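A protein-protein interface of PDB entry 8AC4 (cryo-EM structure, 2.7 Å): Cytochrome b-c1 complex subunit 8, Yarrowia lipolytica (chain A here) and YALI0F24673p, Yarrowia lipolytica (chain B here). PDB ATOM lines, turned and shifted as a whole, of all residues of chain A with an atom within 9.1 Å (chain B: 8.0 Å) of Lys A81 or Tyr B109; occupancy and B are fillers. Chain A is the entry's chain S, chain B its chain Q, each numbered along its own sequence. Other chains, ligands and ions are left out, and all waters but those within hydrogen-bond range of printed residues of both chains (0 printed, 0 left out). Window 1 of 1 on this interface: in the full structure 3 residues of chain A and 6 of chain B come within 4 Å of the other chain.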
ATOM      1  N   GLU A  76      -2.890  -0.644 -10.156  1.00  0.00           N
ATOM      2  CA  GLU A  76      -1.606   0.031 -10.112  1.00  0.00           C
ATOM      3  C   GLU A  76      -0.740  -0.475 -11.261  1.00  0.00           C
ATOM      4  O   GLU A  76      -0.050   0.308 -11.906  1.00  0.00           O
ATOM      5  CB  GLU A  76      -0.937  -0.123  -8.742  1.00  0.00           C
ATOM      6  CG  GLU A  76       0.566   0.130  -8.739  1.00  0.00           C
ATOM      7  CD  GLU A  76       1.148   0.741  -7.470  1.00  0.00           C
ATOM      8  OE1 GLU A  76       0.365   1.309  -6.679  1.00  0.00           O
ATOM      9  OE2 GLU A  76       2.387   0.656  -7.277  1.00  0.00           O
ATOM     10  N   TRP A  77      -0.812  -1.782 -11.508  1.00  0.00           N
ATOM     11  CA  TRP A  77       0.041  -2.423 -12.486  1.00  0.00           C
ATOM     12  C   TRP A  77      -0.397  -2.070 -13.904  1.00  0.00           C
ATOM     13  O   TRP A  77       0.438  -1.994 -14.800  1.00  0.00           O
ATOM     14  CB  TRP A  77       0.053  -3.932 -12.247  1.00  0.00           C
ATOM     15  CG  TRP A  77       0.915  -4.654 -13.230  1.00  0.00           C
ATOM     16  CD1 TRP A  77       2.269  -4.816 -13.172  1.00  0.00           C
ATOM     17  CD2 TRP A  77       0.480  -5.286 -14.442  1.00  0.00           C
ATOM     18  NE1 TRP A  77       2.709  -5.517 -14.261  1.00  0.00           N
ATOM     19  CE2 TRP A  77       1.635  -5.818 -15.058  1.00  0.00           C
ATOM     20  CE3 TRP A  77      -0.766  -5.450 -15.060  1.00  0.00           C
ATOM     21  CZ2 TRP A  77       1.576  -6.511 -16.266  1.00  0.00           C
ATOM     22  CZ3 TRP A  77      -0.823  -6.147 -16.248  1.00  0.00           C
ATOM     23  CH2 TRP A  77       0.333  -6.666 -16.840  1.00  0.00           C
ATOM     24  N   LEU A  78      -1.699  -1.854 -14.108  1.00  0.00           N
ATOM     25  CA  LEU A  78      -2.213  -1.560 -15.439  1.00  0.00           C
ATOM     26  C   LEU A  78      -1.730  -0.196 -15.914  1.00  0.00           C
ATOM     27  O   LEU A  78      -1.683   0.064 -17.113  1.00  0.00           O
ATOM     28  CB  LEU A  78      -3.739  -1.541 -15.388  1.00  0.00           C
ATOM     29  CG  LEU A  78      -4.401  -2.910 -15.435  1.00  0.00           C
ATOM     30  CD1 LEU A  78      -5.905  -2.785 -15.237  1.00  0.00           C
ATOM     31  CD2 LEU A  78      -4.089  -3.600 -16.752  1.00  0.00           C
ATOM     32  N   TYR A  79      -1.436   0.692 -14.961  1.00  0.00           N
ATOM     33  CA  TYR A  79      -1.052   2.050 -15.297  1.00  0.00           C
ATOM     34  C   TYR A  79       0.459   2.218 -15.172  1.00  0.00           C
ATOM     35  O   TYR A  79       0.948   3.331 -14.993  1.00  0.00           O
ATOM     36  CB  TYR A  79      -1.882   3.042 -14.481  1.00  0.00           C
ATOM     37  CG  TYR A  79      -3.298   3.162 -14.980  1.00  0.00           C
ATOM     38  CD1 TYR A  79      -3.638   4.104 -15.937  1.00  0.00           C
ATOM     39  CD2 TYR A  79      -4.287   2.297 -14.536  1.00  0.00           C
ATOM     40  CE1 TYR A  79      -4.932   4.204 -16.425  1.00  0.00           C
ATOM     41  CE2 TYR A  79      -5.587   2.385 -15.011  1.00  0.00           C
ATOM     42  CZ  TYR A  79      -5.909   3.339 -15.960  1.00  0.00           C
ATOM     43  OH  TYR A  79      -7.181   3.438 -16.443  1.00  0.00           O
ATOM     44  N   THR A  80       1.184   1.098 -15.248  1.00  0.00           N
ATOM     45  CA  THR A  80       2.623   1.139 -15.452  1.00  0.00           C
ATOM     46  C   THR A  80       2.906   0.908 -16.935  1.00  0.00           C
ATOM     47  O   THR A  80       1.979   0.681 -17.713  1.00  0.00           O
ATOM     48  CB  THR A  80       3.353   0.171 -14.510  1.00  0.00           C
ATOM     49  OG1 THR A  80       2.986  -1.167 -14.841  1.00  0.00           O
ATOM     50  CG2 THR A  80       3.076   0.431 -13.044  1.00  0.00           C
ATOM     51  N   LYS A  81       4.192   0.987 -17.305  1.00  0.00           N
ATOM     52  CA  LYS A  81       4.681   0.719 -18.649  1.00  0.00           C
ATOM     53  C   LYS A  81       4.445  -0.745 -19.003  1.00  0.00           C
ATOM     54  O   LYS A  81       4.032  -1.065 -20.116  1.00  0.00           O
ATOM     55  CB  LYS A  81       6.194   0.935 -18.699  1.00  0.00           C
ATOM     56  CG  LYS A  81       6.668   2.290 -19.192  1.00  0.00           C
ATOM     57  CD  LYS A  81       8.172   2.311 -19.355  1.00  0.00           C
ATOM     58  CE  LYS A  81       8.814   3.509 -18.692  1.00  0.00           C
ATOM     59  NZ  LYS A  81      10.292   3.392 -18.670  1.00  0.00           N
ATOM     60  N   ALA A  82       4.748  -1.622 -18.038  1.00  0.00           N
ATOM     61  CA  ALA A  82       4.622  -3.063 -18.176  1.00  0.00           C
ATOM     62  C   ALA A  82       3.171  -3.461 -18.450  1.00  0.00           C
ATOM     63  O   ALA A  82       2.920  -4.478 -19.096  1.00  0.00           O
ATOM     64  CB  ALA A  82       5.147  -3.723 -16.926  1.00  0.00           C
ATOM     65  N   GLY A  83       2.229  -2.643 -17.969  1.00  0.00           N
ATOM     66  CA  GLY A  83       0.816  -2.976 -18.032  1.00  0.00           C
ATOM     67  C   GLY A  83       0.085  -2.313 -19.196  1.00  0.00           C
ATOM     68  O   GLY A  83      -1.148  -2.312 -19.215  1.00  0.00           O
ATOM     69  N   ARG A  84       0.856  -1.767 -20.151  1.00  0.00           N
ATOM     70  CA  ARG A  84       0.343  -0.963 -21.252  1.00  0.00           C
ATOM     71  C   ARG A  84      -0.658  -1.752 -22.082  1.00  0.00           C
ATOM     72  O   ARG A  84      -1.695  -1.225 -22.485  1.00  0.00           O
ATOM     73  CB  ARG A  84       1.460  -0.647 -22.243  1.00  0.00           C
ATOM     74  CG  ARG A  84       2.113   0.707 -22.031  1.00  0.00           C
ATOM     75  CD  ARG A  84       2.916   1.004 -23.278  1.00  0.00           C
ATOM     76  NE  ARG A  84       4.032   0.086 -23.482  1.00  0.00           N
ATOM     77  CZ  ARG A  84       4.386  -0.431 -24.655  1.00  0.00           C
ATOM     78  NH1 ARG A  84       3.702  -0.141 -25.750  1.00  0.00           N
ATOM     79  NH2 ARG A  84       5.421  -1.250 -24.725  1.00  0.00           N
ATOM     80  N   HIS A  85      -0.282  -2.998 -22.373  1.00  0.00           N
ATOM     81  CA  HIS A  85      -0.990  -3.829 -23.323  1.00  0.00           C
ATOM     82  C   HIS A  85      -2.291  -4.312 -22.706  1.00  0.00           C
ATOM     83  O   HIS A  85      -3.326  -4.355 -23.369  1.00  0.00           O
ATOM     84  CB  HIS A  85      -0.124  -5.030 -23.708  1.00  0.00           C
ATOM     85  CG  HIS A  85       1.184  -4.640 -24.304  1.00  0.00           C
ATOM     86  ND1 HIS A  85       1.274  -3.981 -25.515  1.00  0.00           N
ATOM     87  CD2 HIS A  85       2.449  -4.804 -23.862  1.00  0.00           C
ATOM     88  CE1 HIS A  85       2.543  -3.760 -25.797  1.00  0.00           C
ATOM     89  NE2 HIS A  85       3.284  -4.256 -24.798  1.00  0.00           N
ATOM     90  N   GLU A  86      -2.188  -4.717 -21.435  1.00  0.00           N
ATOM     91  CA  GLU A  86      -3.320  -5.232 -20.692  1.00  0.00           C
ATOM     92  C   GLU A  86      -4.305  -4.094 -20.452  1.00  0.00           C
ATOM     93  O   GLU A  86      -5.504  -4.340 -20.350  1.00  0.00           O
ATOM     94  CB  GLU A  86      -2.885  -5.895 -19.382  1.00  0.00           C
ATOM     95  CG  GLU A  86      -2.227  -7.258 -19.554  1.00  0.00           C
ATOM     96  CD  GLU A  86      -0.834  -7.292 -20.170  1.00  0.00           C
ATOM     97  OE1 GLU A  86      -0.084  -6.299 -20.022  1.00  0.00           O
ATOM     98  OE2 GLU A  86      -0.502  -8.312 -20.810  1.00  0.00           O
ATOM     99  N   LEU A  87      -3.787  -2.862 -20.358  1.00  0.00           N
ATOM    100  CA  LEU A  87      -4.654  -1.717 -20.133  1.00  0.00           C
ATOM    101  C   LEU A  87      -5.400  -1.388 -21.420  1.00  0.00           C
ATOM    102  O   LEU A  87      -6.540  -0.939 -21.372  1.00  0.00           O
ATOM    103  CB  LEU A  87      -3.852  -0.506 -19.649  1.00  0.00           C
ATOM    104  CG  LEU A  87      -4.663   0.777 -19.460  1.00  0.00           C
ATOM    105  CD1 LEU A  87      -5.686   0.633 -18.339  1.00  0.00           C
ATOM    106  CD2 LEU A  87      -3.758   1.972 -19.209  1.00  0.00           C
ATOM    107  N   HIS B  87      18.350   1.347 -12.545  1.00  0.00           N
ATOM    108  CA  HIS B  87      17.177   1.222 -13.402  1.00  0.00           C
ATOM    109  C   HIS B  87      16.969   2.497 -14.211  1.00  0.00           C
ATOM    110  O   HIS B  87      16.734   2.439 -15.418  1.00  0.00           O
ATOM    111  CB  HIS B  87      15.913   0.904 -12.599  1.00  0.00           C
ATOM    112  CG  HIS B  87      15.920  -0.467 -12.018  1.00  0.00           C
ATOM    113  ND1 HIS B  87      15.235  -0.769 -10.865  1.00  0.00           N
ATOM    114  CD2 HIS B  87      16.541  -1.605 -12.402  1.00  0.00           C
ATOM    115  CE1 HIS B  87      15.423  -2.035 -10.559  1.00  0.00           C
ATOM    116  NE2 HIS B  87      16.222  -2.571 -11.490  1.00  0.00           N
ATOM    117  N   PHE B  88      17.027   3.637 -13.515  1.00  0.00           N
ATOM    118  CA  PHE B  88      16.864   4.929 -14.147  1.00  0.00           C
ATOM    119  C   PHE B  88      17.933   5.124 -15.221  1.00  0.00           C
ATOM    120  O   PHE B  88      17.612   5.539 -16.335  1.00  0.00           O
ATOM    121  CB  PHE B  88      16.854   6.042 -13.099  1.00  0.00           C
ATOM    122  CG  PHE B  88      16.673   7.420 -13.678  1.00  0.00           C
ATOM    123  CD1 PHE B  88      15.563   7.726 -14.458  1.00  0.00           C
ATOM    124  CD2 PHE B  88      17.617   8.411 -13.451  1.00  0.00           C
ATOM    125  CE1 PHE B  88      15.403   8.993 -15.002  1.00  0.00           C
ATOM    126  CE2 PHE B  88      17.444   9.686 -13.974  1.00  0.00           C
ATOM    127  CZ  PHE B  88      16.341   9.972 -14.752  1.00  0.00           C
ATOM    128  N   CYS B  91      17.258   2.967 -18.243  1.00  0.00           N
ATOM    129  CA  CYS B  91      16.141   3.569 -18.953  1.00  0.00           C
ATOM    130  C   CYS B  91      16.629   4.735 -19.808  1.00  0.00           C
ATOM    131  O   CYS B  91      16.300   4.771 -20.994  1.00  0.00           O
ATOM    132  CB  CYS B  91      15.029   4.031 -18.016  1.00  0.00           C
ATOM    133  SG  CYS B  91      13.588   4.755 -18.852  1.00  0.00           S
ATOM    134  N   VAL B  92      17.406   5.660 -19.214  1.00  0.00           N
ATOM    135  CA  VAL B  92      17.804   6.853 -19.946  1.00  0.00           C
ATOM    136  C   VAL B  92      18.623   6.459 -21.174  1.00  0.00           C
ATOM    137  O   VAL B  92      18.352   6.973 -22.259  1.00  0.00           O
ATOM    138  CB  VAL B  92      18.423   7.989 -19.106  1.00  0.00           C
ATOM    139  CG1 VAL B  92      17.511   8.480 -17.995  1.00  0.00           C
ATOM    140  CG2 VAL B  92      19.816   7.691 -18.595  1.00  0.00           C
ATOM    141  N   ARG B  94      18.396   3.732 -22.953  1.00  0.00           N
ATOM    142  CA  ARG B  94      17.481   3.197 -23.955  1.00  0.00           C
ATOM    143  C   ARG B  94      16.738   4.320 -24.668  1.00  0.00           C
ATOM    144  O   ARG B  94      16.610   4.286 -25.891  1.00  0.00           O
ATOM    145  CB  ARG B  94      16.465   2.219 -23.356  1.00  0.00           C
ATOM    146  CG  ARG B  94      17.090   0.935 -22.829  1.00  0.00           C
ATOM    147  CD  ARG B  94      16.183  -0.028 -22.089  1.00  0.00           C
ATOM    148  NE  ARG B  94      15.495   0.516 -20.920  1.00  0.00           N
ATOM    149  CZ  ARG B  94      14.175   0.648 -20.832  1.00  0.00           C
ATOM    150  NH1 ARG B  94      13.415   0.261 -21.843  1.00  0.00           N
ATOM    151  NH2 ARG B  94      13.634   1.139 -19.732  1.00  0.00           N
ATOM    152  N   VAL B  95      16.248   5.295 -23.900  1.00  0.00           N
ATOM    153  CA  VAL B  95      15.376   6.315 -24.455  1.00  0.00           C
ATOM    154  C   VAL B  95      16.181   7.257 -25.349  1.00  0.00           C
ATOM    155  O   VAL B  95      15.737   7.565 -26.454  1.00  0.00           O
ATOM    156  CB  VAL B  95      14.554   7.033 -23.368  1.00  0.00           C
ATOM    157  CG1 VAL B  95      13.860   8.281 -23.895  1.00  0.00           C
ATOM    158  CG2 VAL B  95      13.523   6.087 -22.774  1.00  0.00           C
ATOM    159  N   ALA B  98      16.914   5.612 -28.507  1.00  0.00           N
ATOM    160  CA  ALA B  98      15.707   5.457 -29.300  1.00  0.00           C
ATOM    161  C   ALA B  98      15.378   6.770 -30.004  1.00  0.00           C
ATOM    162  O   ALA B  98      14.827   6.765 -31.104  1.00  0.00           O
ATOM    163  CB  ALA B  98      14.570   4.990 -28.426  1.00  0.00           C
ATOM    164  N   TYR B 104      11.705   8.275 -35.250  1.00  0.00           N
ATOM    165  CA  TYR B 104      11.260   8.213 -33.870  1.00  0.00           C
ATOM    166  C   TYR B 104      10.044   9.122 -33.691  1.00  0.00           C
ATOM    167  O   TYR B 104       9.144   8.810 -32.913  1.00  0.00           O
ATOM    168  CB  TYR B 104      12.408   8.542 -32.904  1.00  0.00           C
ATOM    169  CG  TYR B 104      11.956   8.884 -31.505  1.00  0.00           C
ATOM    170  CD1 TYR B 104      11.626   7.892 -30.591  1.00  0.00           C
ATOM    171  CD2 TYR B 104      11.810  10.206 -31.106  1.00  0.00           C
ATOM    172  CE1 TYR B 104      11.169   8.204 -29.317  1.00  0.00           C
ATOM    173  CE2 TYR B 104      11.354  10.535 -29.840  1.00  0.00           C
ATOM    174  CZ  TYR B 104      11.035   9.532 -28.940  1.00  0.00           C
ATOM    175  OH  TYR B 104      10.609   9.862 -27.684  1.00  0.00           O
ATOM    176  N   HIS B 106       7.790   9.733 -35.855  1.00  0.00           N
ATOM    177  CA  HIS B 106       6.653   9.061 -36.468  1.00  0.00           C
ATOM    178  C   HIS B 106       6.508   7.648 -35.902  1.00  0.00           C
ATOM    179  O   HIS B 106       6.254   6.700 -36.645  1.00  0.00           O
ATOM    180  CB  HIS B 106       6.759   9.085 -38.003  1.00  0.00           C
ATOM    181  CG  HIS B 106       6.718  10.457 -38.592  1.00  0.00           C
ATOM    182  ND1 HIS B 106       5.565  11.222 -38.618  1.00  0.00           N
ATOM    183  CD2 HIS B 106       7.680  11.205 -39.175  1.00  0.00           C
ATOM    184  CE1 HIS B 106       5.822  12.383 -39.190  1.00  0.00           C
ATOM    185  NE2 HIS B 106       7.114  12.398 -39.541  1.00  0.00           N
ATOM    186  N   ALA B 107       6.676   7.522 -34.581  1.00  0.00           N
ATOM    187  CA  ALA B 107       6.418   6.272 -33.883  1.00  0.00           C
ATOM    188  C   ALA B 107       5.124   6.402 -33.082  1.00  0.00           C
ATOM    189  O   ALA B 107       4.672   7.514 -32.793  1.00  0.00           O
ATOM    190  CB  ALA B 107       7.602   5.881 -33.025  1.00  0.00           C
ATOM    191  N   GLU B 108       4.529   5.254 -32.750  1.00  0.00           N
ATOM    192  CA  GLU B 108       3.259   5.229 -32.046  1.00  0.00           C
ATOM    193  C   GLU B 108       3.496   5.530 -30.565  1.00  0.00           C
ATOM    194  O   GLU B 108       2.905   6.463 -30.013  1.00  0.00           O
ATOM    195  CB  GLU B 108       2.537   3.904 -32.325  1.00  0.00           C
ATOM    196  CG  GLU B 108       1.051   3.914 -31.977  1.00  0.00           C
ATOM    197  CD  GLU B 108       0.704   3.732 -30.506  1.00  0.00           C
ATOM    198  OE1 GLU B 108       0.016   4.614 -29.944  1.00  0.00           O
ATOM    199  OE2 GLU B 108       1.110   2.702 -29.925  1.00  0.00           O
ATOM    200  N   TYR B 109       4.386   4.740 -29.946  1.00  0.00           N
ATOM    201  CA  TYR B 109       4.680   4.833 -28.525  1.00  0.00           C
ATOM    202  C   TYR B 109       6.081   5.401 -28.306  1.00  0.00           C
ATOM    203  O   TYR B 109       7.070   4.798 -28.715  1.00  0.00           O
ATOM    204  CB  TYR B 109       4.524   3.464 -27.850  1.00  0.00           C
ATOM    205  CG  TYR B 109       5.011   3.403 -26.423  1.00  0.00           C
ATOM    206  CD1 TYR B 109       4.380   4.131 -25.421  1.00  0.00           C
ATOM    207  CD2 TYR B 109       6.109   2.629 -26.069  1.00  0.00           C
ATOM    208  CE1 TYR B 109       4.820   4.085 -24.105  1.00  0.00           C
ATOM    209  CE2 TYR B 109       6.565   2.578 -24.759  1.00  0.00           C
ATOM    210  CZ  TYR B 109       5.915   3.305 -23.772  1.00  0.00           C
ATOM    211  OH  TYR B 109       6.350   3.255 -22.477  1.00  0.00           O
ATOM    212  N   LYS B 110       6.145   6.547 -27.621  1.00  0.00           N
ATOM    213  CA  LYS B 110       7.406   7.128 -27.187  1.00  0.00           C
ATOM    214  C   LYS B 110       7.591   6.899 -25.687  1.00  0.00           C
ATOM    215  O   LYS B 110       6.833   7.420 -24.869  1.00  0.00           O
ATOM    216  CB  LYS B 110       7.455   8.610 -27.565  1.00  0.00           C
ATOM    217  CG  LYS B 110       7.357   8.911 -29.057  1.00  0.00           C
ATOM    218  CD  LYS B 110       7.175  10.390 -29.340  1.00  0.00           C
ATOM    219  CE  LYS B 110       7.229  10.762 -30.809  1.00  0.00           C
ATOM    220  NZ  LYS B 110       6.203  10.066 -31.619  1.00  0.00           N
ATOM    221  N   GLU B 111       8.609   6.101 -25.342  1.00  0.00           N
ATOM    222  CA  GLU B 111       8.931   5.756 -23.963  1.00  0.00           C
ATOM    223  C   GLU B 111       9.551   6.962 -23.252  1.00  0.00           C
ATOM    224  O   GLU B 111      10.380   7.657 -23.835  1.00  0.00           O
ATOM    225  CB  GLU B 111       9.908   4.580 -23.953  1.00  0.00           C
ATOM    226  CG  GLU B 111       9.881   3.795 -22.659  1.00  0.00           C
ATOM    227  CD  GLU B 111      11.041   2.873 -22.336  1.00  0.00           C
ATOM    228  OE1 GLU B 111      11.209   2.594 -21.141  1.00  0.00           O
ATOM    229  OE2 GLU B 111      11.755   2.422 -23.260  1.00  0.00           O
ATOM    230  N   ASP B 112       9.157   7.188 -21.983  1.00  0.00           N
ATOM    231  CA  ASP B 112       9.842   8.112 -21.086  1.00  0.00           C
ATOM    232  C   ASP B 112      10.546   7.340 -19.969  1.00  0.00           C
ATOM    233  O   ASP B 112      10.519   6.112 -19.945  1.00  0.00           O
ATOM    234  CB  ASP B 112       8.877   9.149 -20.508  1.00  0.00           C
ATOM    235  CG  ASP B 112       7.666   8.526 -19.832  1.00  0.00           C
ATOM    236  OD1 ASP B 112       7.769   8.146 -18.642  1.00  0.00           O
ATOM    237  OD2 ASP B 112       6.642   8.376 -20.526  1.00  0.00           O
ATOM    238  N   CYS B 113      11.137   8.079 -19.026  1.00  0.00           N
ATOM    239  CA  CYS B 113      11.791   7.461 -17.887  1.00  0.00           C
ATOM    240  C   CYS B 113      11.210   7.965 -16.577  1.00  0.00           C
ATOM    241  O   CYS B 113      11.849   7.865 -15.528  1.00  0.00           O
ATOM    242  CB  CYS B 113      13.288   7.708 -17.946  1.00  0.00           C
ATOM    243  SG  CYS B 113      14.027   6.723 -19.271  1.00  0.00           S
ATOM    244  N   VAL B 114       9.975   8.449 -16.651  1.00  0.00           N
ATOM    245  CA  VAL B 114       9.369   9.094 -15.504  1.00  0.00           C
ATOM    246  C   VAL B 114       9.125   8.063 -14.411  1.00  0.00           C
ATOM    247  O   VAL B 114       9.426   8.329 -13.251  1.00  0.00           O
ATOM    248  CB  VAL B 114       8.101   9.851 -15.918  1.00  0.00           C
ATOM    249  CG1 VAL B 114       7.195  10.180 -14.746  1.00  0.00           C
ATOM    250  CG2 VAL B 114       8.484  11.101 -16.665  1.00  0.00           C
ATOM    251  N   GLU B 115       8.649   6.876 -14.797  1.00  0.00           N
ATOM    252  CA  GLU B 115       8.371   5.828 -13.826  1.00  0.00           C
ATOM    253  C   GLU B 115       9.603   5.518 -12.982  1.00  0.00           C
ATOM    254  O   GLU B 115       9.529   5.483 -11.756  1.00  0.00           O
ATOM    255  CB  GLU B 115       7.869   4.564 -14.513  1.00  0.00           C
ATOM    256  CG  GLU B 115       6.384   4.342 -14.321  1.00  0.00           C
ATOM    257  CD  GLU B 115       5.786   3.258 -15.204  1.00  0.00           C
ATOM    258  OE1 GLU B 115       6.188   2.082 -15.057  1.00  0.00           O
ATOM    259  OE2 GLU B 115       4.923   3.594 -16.046  1.00  0.00           O
ATOM    260  N   GLU B 116      10.734   5.311 -13.662  1.00  0.00           N
ATOM    261  CA  GLU B 116      11.979   4.927 -13.018  1.00  0.00           C
ATOM    262  C   GLU B 116      12.497   6.082 -12.173  1.00  0.00           C
ATOM    263  O   GLU B 116      13.091   5.873 -11.114  1.00  0.00           O
ATOM    264  CB  GLU B 116      13.032   4.563 -14.063  1.00  0.00           C
ATOM    265  CG  GLU B 116      12.843   3.180 -14.640  1.00  0.00           C
ATOM    266  CD  GLU B 116      11.826   3.073 -15.766  1.00  0.00           C
ATOM    267  OE1 GLU B 116      11.564   1.942 -16.204  1.00  0.00           O
ATOM    268  OE2 GLU B 116      11.256   4.119 -16.153  1.00  0.00           O
ATOM    269  N   PHE B 117      12.287   7.295 -12.686  1.00  0.00           N
ATOM    270  CA  PHE B 117      12.688   8.486 -11.971  1.00  0.00           C
ATOM    271  C   PHE B 117      11.914   8.584 -10.659  1.00  0.00           C
ATOM    272  O   PHE B 117      12.514   8.812  -9.609  1.00  0.00           O
ATOM    273  CB  PHE B 117      12.529   9.704 -12.875  1.00  0.00           C
ATOM    274  CG  PHE B 117      12.993  10.973 -12.220  1.00  0.00           C
ATOM    275  CD1 PHE B 117      14.346  11.206 -12.013  1.00  0.00           C
ATOM    276  CD2 PHE B 117      12.077  11.922 -11.791  1.00  0.00           C
ATOM    277  CE1 PHE B 117      14.774  12.378 -11.407  1.00  0.00           C
ATOM    278  CE2 PHE B 117      12.506  13.095 -11.188  1.00  0.00           C
ATOM    279  CZ  PHE B 117      13.854  13.321 -10.997  1.00  0.00           C
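The side-chain sulfur (SG) of Cys B91 sits at hydrogen-bond distance from the side-chain amino group (NZ) of Lys A81. N of Lys A81 lies within hydrogen-bond range of OE2 of Glu B115, at 3.0 Å. The backbone carbonyl oxygen (O) of Asp B112 is in hydrogen-bond range of the side-chain amino group (NZ) of Lys A81 (3.0 Å). The side-chain carboxylate (OE1) of Glu B111 lies within salt-bridge range of the side-chain amino group (NZ) of Lys A81 (2.8 Å). The side-chain carboxylate of Glu B116 is in salt-bridge range of the side-chain amino group of Lys A81 (2.8 Å).
Among the printed residues, pairs that only touch across the chains: Thr A80 with Glu B115 (3.4 Å), Lys A81 with Tyr B109 (3.4 Å) and Arg A84 with Tyr B109 (3.7 Å).
Of the printed residues of chain B, Lys A81 touches Cys B91, Tyr B109, Glu B111, Asp B112, Glu B115 and Glu B116. Of chain A, only Lys A81 (3.4 Å) and Arg A84 (3.7 Å) come within 4 Å of Tyr B109. No residue of chain A comes within 4 Å of Glu B108. Printed residues of chain B within 4 Å of Arg A84: Tyr B109 (3.7 Å). Printed residues of chain A within 4 Å of Cys B91: Lys A81 (3.6 Å). Printed residues of chain A within 4 Å of Glu B111: Lys A81. Of the printed residues of chain A, Glu B116 touches Lys A81 (2.8 Å). Of the printed residues of chain B, Thr A80 touches Glu B115 (3.4 Å). Cys B113 touches none of the printed residues of chain A. Ala B98 touches none of the printed residues of chain A. The nearest residue of chain A that does not touch Tyr B109 is Ala A82 (6.8 Å).
Among the printed residues, Asp or Glu carboxylates within 4 Å of a Lys or Arg side-chain nitrogen of the other chain: Lys A81 with Glu B111 and Lys A81 with Glu B116.
NH1 of Arg B94 lies within salt-bridge range of OE2 of Glu B111, at 3.1 Å. The side-chain sulfur (SG) of Cys B113 forms a disulfide with the side-chain sulfur (SG) of Cys B91 (2.1 Å). OD1 of Asp B112 lies within hydrogen-bond range of N of Val B114 (3.0 Å). NH2 of Arg B94 lies close to SG of Cys B91 (3.7 Å). The backbone carbonyl oxygen (O) of Trp A77 lies within hydrogen-bond range of the side-chain hydroxyl (OG1) of Thr A80 (2.7 Å).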
